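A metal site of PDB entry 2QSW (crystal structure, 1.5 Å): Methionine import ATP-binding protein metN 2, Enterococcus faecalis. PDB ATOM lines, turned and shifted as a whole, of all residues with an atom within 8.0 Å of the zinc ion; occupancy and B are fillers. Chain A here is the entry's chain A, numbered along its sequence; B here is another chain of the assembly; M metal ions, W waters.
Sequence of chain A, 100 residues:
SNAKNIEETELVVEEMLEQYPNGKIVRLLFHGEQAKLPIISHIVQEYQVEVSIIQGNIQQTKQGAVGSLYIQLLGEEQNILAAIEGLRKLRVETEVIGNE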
ATOM      1  N   LEU A  28      26.946 -28.549  -3.627  1.00  0.00           N
ATOM      2  CA  LEU A  28      25.931 -28.035  -4.526  1.00  0.00           C
ATOM      3  C   LEU A  28      26.629 -27.804  -5.863  1.00  0.00           C
ATOM      4  O   LEU A  28      27.681 -27.157  -5.890  1.00  0.00           O
ATOM      5  CB  LEU A  28      25.379 -26.679  -4.025  1.00  0.00           C
ATOM      6  CG  LEU A  28      24.323 -26.647  -2.898  1.00  0.00           C
ATOM      7  CD1 LEU A  28      24.847 -27.238  -1.563  1.00  0.00           C
ATOM      8  CD2 LEU A  28      23.843 -25.210  -2.696  1.00  0.00           C
ATOM      9  N   LEU A  29      25.999 -28.258  -6.952  1.00  0.00           N
ATOM     10  CA  LEU A  29      26.482 -28.001  -8.327  1.00  0.00           C
ATOM     11  C   LEU A  29      25.527 -27.103  -9.087  1.00  0.00           C
ATOM     12  O   LEU A  29      24.288 -27.262  -8.973  1.00  0.00           O
ATOM     13  CB  LEU A  29      26.611 -29.325  -9.101  1.00  0.00           C
ATOM     14  CG  LEU A  29      27.551 -30.350  -8.507  1.00  0.00           C
ATOM     15  CD1 LEU A  29      27.624 -31.661  -9.387  1.00  0.00           C
ATOM     16  CD2 LEU A  29      28.930 -29.747  -8.200  1.00  0.00           C
ATOM     17  N   PHE A  30      26.096 -26.139  -9.835  1.00  0.00           N
ATOM     18  CA  PHE A  30      25.342 -25.150 -10.615  1.00  0.00           C
ATOM     19  C   PHE A  30      25.807 -25.298 -12.039  1.00  0.00           C
ATOM     20  O   PHE A  30      27.000 -25.228 -12.304  1.00  0.00           O
ATOM     21  CB  PHE A  30      25.640 -23.728 -10.124  1.00  0.00           C
ATOM     22  CG  PHE A  30      25.237 -23.511  -8.682  1.00  0.00           C
ATOM     23  CD1 PHE A  30      23.948 -23.142  -8.348  1.00  0.00           C
ATOM     24  CD2 PHE A  30      26.129 -23.776  -7.678  1.00  0.00           C
ATOM     25  CE1 PHE A  30      23.559 -22.968  -7.017  1.00  0.00           C
ATOM     26  CE2 PHE A  30      25.750 -23.584  -6.338  1.00  0.00           C
ATOM     27  CZ  PHE A  30      24.489 -23.200  -6.020  1.00  0.00           C
ATOM     28  N   HIS A  31      24.879 -25.629 -12.955  1.00  0.00           N
ATOM     29  CA  HIS A  31      25.213 -25.770 -14.377  1.00  0.00           C
ATOM     30  C   HIS A  31      24.519 -24.701 -15.219  1.00  0.00           C
ATOM     31  O   HIS A  31      24.616 -24.723 -16.448  1.00  0.00           O
ATOM     32  CB  HIS A  31      24.792 -27.145 -14.901  1.00  0.00           C
ATOM     33  CG  HIS A  31      25.358 -28.288 -14.120  1.00  0.00           C
ATOM     34  ND1 HIS A  31      24.697 -28.912 -13.046  1.00  0.00           N
ATOM     35  CD2 HIS A  31      26.535 -28.943 -14.281  1.00  0.00           C
ATOM     36  CE1 HIS A  31      25.464 -29.888 -12.596  1.00  0.00           C
ATOM     37  NE2 HIS A  31      26.581 -29.929 -13.321  1.00  0.00           N
ATOM     38  N   GLY A  32      23.834 -23.769 -14.590  1.00  0.00           N
ATOM     39  CA  GLY A  32      23.087 -22.701 -15.255  1.00  0.00           C
ATOM     40  C   GLY A  32      21.629 -23.004 -15.441  1.00  0.00           C
ATOM     41  O   GLY A  32      20.868 -22.121 -15.873  1.00  0.00           O
ATOM     42  N   GLU A  33      21.226 -24.262 -15.157  1.00  0.00           N
ATOM     43  CA  GLU A  33      19.839 -24.643 -15.233  1.00  0.00           C
ATOM     44  C   GLU A  33      19.048 -24.445 -13.927  1.00  0.00           C
ATOM     45  O   GLU A  33      17.823 -24.595 -13.904  1.00  0.00           O
ATOM     46  CB  GLU A  33      19.707 -26.100 -15.703  1.00  0.00           C
ATOM     47  CG  GLU A  33      19.761 -27.191 -14.644  1.00  0.00           C
ATOM     48  CD  GLU A  33      21.120 -27.467 -13.978  1.00  0.00           C
ATOM     49  OE1 GLU A  33      22.031 -26.587 -13.940  1.00  0.00           O
ATOM     50  OE2 GLU A  33      21.299 -28.577 -13.399  1.00  0.00           O
ATOM     51  N   GLN A  34      19.762 -24.101 -12.860  1.00  0.00           N
ATOM     52  CA  GLN A  34      19.122 -23.924 -11.558  1.00  0.00           C
ATOM     53  C   GLN A  34      18.022 -22.864 -11.566  1.00  0.00           C
ATOM     54  O   GLN A  34      18.030 -21.933 -12.377  1.00  0.00           O
ATOM     55  CB  GLN A  34      20.158 -23.587 -10.484  1.00  0.00           C
ATOM     56  CG  GLN A  34      20.861 -22.249 -10.746  1.00  0.00           C
ATOM     57  CD  GLN A  34      22.197 -22.397 -11.532  1.00  0.00           C
ATOM     58  OE1 GLN A  34      22.483 -23.429 -12.124  1.00  0.00           O
ATOM     59  NE2 GLN A  34      23.005 -21.310 -11.528  1.00  0.00           N
ATOM     60  N   ALA A  65      25.209 -18.810 -13.610  1.00  0.00           N
ATOM     61  CA  ALA A  65      26.214 -19.129 -12.603  1.00  0.00           C
ATOM     62  C   ALA A  65      26.529 -20.605 -12.693  1.00  0.00           C
ATOM     63  O   ALA A  65      25.609 -21.433 -12.706  1.00  0.00           O
ATOM     64  CB  ALA A  65      25.780 -18.794 -11.170  1.00  0.00           C
ATOM     65  N   GLY A  67      29.365 -23.810 -11.394  1.00  0.00           N
ATOM     66  CA  GLY A  67      30.391 -24.245 -10.502  1.00  0.00           C
ATOM     67  C   GLY A  67      29.889 -25.056  -9.318  1.00  0.00           C
ATOM     68  O   GLY A  67      28.857 -25.716  -9.437  1.00  0.00           O
ATOM     69  N   ARG A  88      17.717 -29.926  -4.706  1.00  0.00           N
ATOM     70  CA  ARG A  88      17.650 -30.804  -5.886  1.00  0.00           C
ATOM     71  C   ARG A  88      16.457 -30.467  -6.758  1.00  0.00           C
ATOM     72  O   ARG A  88      16.561 -30.419  -7.980  1.00  0.00           O
ATOM     73  CB  ARG A  88      17.565 -32.255  -5.452  1.00  0.00           C
ATOM     74  CG  ARG A  88      18.894 -32.758  -4.908  1.00  0.00           C
ATOM     75  CD  ARG A  88      18.709 -34.049  -4.181  1.00  0.00           C
ATOM     76  NE  ARG A  88      19.976 -34.549  -3.657  1.00  0.00           N
ATOM     77  CZ  ARG A  88      20.066 -35.482  -2.718  1.00  0.00           C
ATOM     78  NH1 ARG A  88      18.959 -36.033  -2.220  1.00  0.00           N
ATOM     79  NH2 ARG A  88      21.251 -35.862  -2.279  1.00  0.00           N
ATOM     80  N   LEU A  90      14.922 -27.636  -6.961  1.00  0.00           N
ATOM     81  CA  LEU A  90      15.272 -26.341  -7.553  1.00  0.00           C
ATOM     82  C   LEU A  90      16.402 -26.461  -8.598  1.00  0.00           C
ATOM     83  O   LEU A  90      16.880 -25.430  -9.085  1.00  0.00           O
ATOM     84  CB  LEU A  90      15.658 -25.335  -6.463  1.00  0.00           C
ATOM     85  CG  LEU A  90      14.496 -24.992  -5.496  1.00  0.00           C
ATOM     86  CD1 LEU A  90      15.072 -24.119  -4.356  1.00  0.00           C
ATOM     87  CD2 LEU A  90      13.321 -24.314  -6.244  1.00  0.00           C
ATOM     88  N   ARG A  91      16.789 -27.682  -8.984  1.00  0.00           N
ATOM     89  CA  ARG A  91      17.745 -27.970 -10.074  1.00  0.00           C
ATOM     90  C   ARG A  91      19.162 -27.600  -9.695  1.00  0.00           C
ATOM     91  O   ARG A  91      19.998 -27.232 -10.524  1.00  0.00           O
ATOM     92  CB  ARG A  91      17.248 -27.384 -11.403  1.00  0.00           C
ATOM     93  CG  ARG A  91      15.794 -27.818 -11.744  1.00  0.00           C
ATOM     94  CD  ARG A  91      15.071 -27.025 -12.837  1.00  0.00           C
ATOM     95  NE  ARG A  91      15.729 -27.237 -14.120  1.00  0.00           N
ATOM     96  CZ  ARG A  91      15.476 -26.553 -15.244  1.00  0.00           C
ATOM     97  NH1 ARG A  91      14.614 -25.563 -15.259  1.00  0.00           N
ATOM     98  NH2 ARG A  91      16.183 -26.838 -16.341  1.00  0.00           N
ATOM     99  N   VAL A  92      19.450 -27.742  -8.391  1.00  0.00           N
ATOM    100  CA  VAL A  92      20.778 -27.683  -7.870  1.00  0.00           C
ATOM    101  C   VAL A  92      21.135 -29.095  -7.354  1.00  0.00           C
ATOM    102  O   VAL A  92      20.681 -29.506  -6.273  1.00  0.00           O
ATOM    103  CB  VAL A  92      20.898 -26.622  -6.684  1.00  0.00           C
ATOM    104  CG1 VAL A  92      22.297 -26.671  -6.117  1.00  0.00           C
ATOM    105  CG2 VAL A  92      20.506 -25.225  -7.120  1.00  0.00           C
ATOM    106  N   GLU A  93      21.959 -29.799  -8.099  1.00  0.00           N
ATOM    107  CA  GLU A  93      22.389 -31.153  -7.693  1.00  0.00           C
ATOM    108  C   GLU A  93      23.161 -31.051  -6.376  1.00  0.00           C
ATOM    109  O   GLU A  93      24.060 -30.231  -6.231  1.00  0.00           O
ATOM    110  CB  GLU A  93      23.241 -31.808  -8.736  1.00  0.00           C
ATOM    111  CG  GLU A  93      22.527 -32.159 -10.019  1.00  0.00           C
ATOM    112  CD  GLU A  93      22.644 -31.104 -11.121  1.00  0.00           C
ATOM    113  OE1 GLU A  93      22.866 -29.909 -10.784  1.00  0.00           O
ATOM    114  OE2 GLU A  93      22.547 -31.464 -12.300  1.00  0.00           O
ATOM    115  N   THR A  94      22.789 -31.866  -5.397  1.00  0.00           N
ATOM    116  CA  THR A  94      23.291 -31.717  -4.043  1.00  0.00           C
ATOM    117  C   THR A  94      23.550 -33.099  -3.484  1.00  0.00           C
ATOM    118  O   THR A  94      22.743 -34.009  -3.630  1.00  0.00           O
ATOM    119  CB  THR A  94      22.255 -30.969  -3.192  1.00  0.00           C
ATOM    120  OG1 THR A  94      21.944 -29.688  -3.781  1.00  0.00           O
ATOM    121  CG2 THR A  94      22.783 -30.735  -1.770  1.00  0.00           C
ATOM    122  N   GLY B  98      23.020 -39.459  -9.378  1.00  0.00           N
ATOM    123  CA  GLY B  98      22.618 -38.348 -10.270  1.00  0.00           C
ATOM    124  C   GLY B  98      22.899 -36.954  -9.760  1.00  0.00           C
ATOM    125  O   GLY B  98      22.367 -35.954 -10.322  1.00  0.00           O
ATOM    126  N   ASN B  99      23.697 -36.883  -8.705  1.00  0.00           N
ATOM    127  CA  ASN B  99      24.074 -35.571  -8.138  1.00  0.00           C
ATOM    128  C   ASN B  99      25.540 -35.224  -8.297  1.00  0.00           C
ATOM    129  O   ASN B  99      26.037 -34.307  -7.615  1.00  0.00           O
ATOM    130  CB  ASN B  99      23.614 -35.465  -6.675  1.00  0.00           C
ATOM    131  CG  ASN B  99      22.110 -35.364  -6.579  1.00  0.00           C
ATOM    132  OD1 ASN B  99      21.513 -34.314  -6.816  1.00  0.00           O
ATOM    133  ND2 ASN B  99      21.463 -36.499  -6.311  1.00  0.00           N
ATOM    134  N   GLU B 100      26.210 -35.882  -9.247  1.00  0.00           N
ATOM    135  CA  GLU B 100      27.573 -35.531  -9.579  1.00  0.00           C
ATOM    136  C   GLU B 100      27.485 -34.766 -10.917  1.00  0.00           C
ATOM    137  O   GLU B 100      28.460 -34.158 -11.357  1.00  0.00           O
ATOM    138  CB  GLU B 100      28.499 -36.757  -9.689  1.00  0.00           C
ATOM    139  CG  GLU B 100      28.203 -38.047  -8.855  1.00  0.00           C
ATOM    140  CD  GLU B 100      28.956 -38.196  -7.492  1.00  0.00           C
ATOM    141  OE1 GLU B 100      28.728 -39.181  -6.775  1.00  0.00           O
ATOM    142  OE2 GLU B 100      29.777 -37.363  -7.103  1.00  0.00           O
ATOM    143  OXT GLU B 100      26.436 -34.698 -11.623  1.00  0.00           O
HETATM  144 ZN    ZN M   1      22.915 -28.679 -12.331  1.00  0.00          ZN
HETATM  145  O   HOH W   1      22.639 -27.005 -11.062  1.00  0.00           O
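The zinc ion is bound by a ring nitrogen (ND1) of His 31 (1.9 Å), the side-chain carboxylate of Glu 33 (1.9 Å), the side-chain carboxylate of Glu 93 (2.0 Å) and water W1 (2.1 Å). The zinc ion has four donor atoms within binding distance. Slightly farther from the zinc ion lies OE1 of Glu 33 (2.8 Å). Slightly farther from the zinc ion lies OE2 of Glu 93 (2.8 Å).
O of Leu 29 touches the zinc ion (3.9 Å). Arg 91 touches the zinc ion (O to ZN, 3.7 Å). Five residues have an atom within 4 Å of the zinc ion: Leu 29, His 31, Glu 33, Arg 91 and Glu 93.
The backbone NH (N) of His 31 lies within hydrogen-bond range of the side-chain amide oxygen (OE1) of Gln 34 (3.4 Å). The backbone carbonyl oxygen (O) of Glu 33 lies close to the guanidinium group (NE) of Arg 91. O of Glu 93 is in hydrogen-bond range of N of Leu 29, 2.9 Å away.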
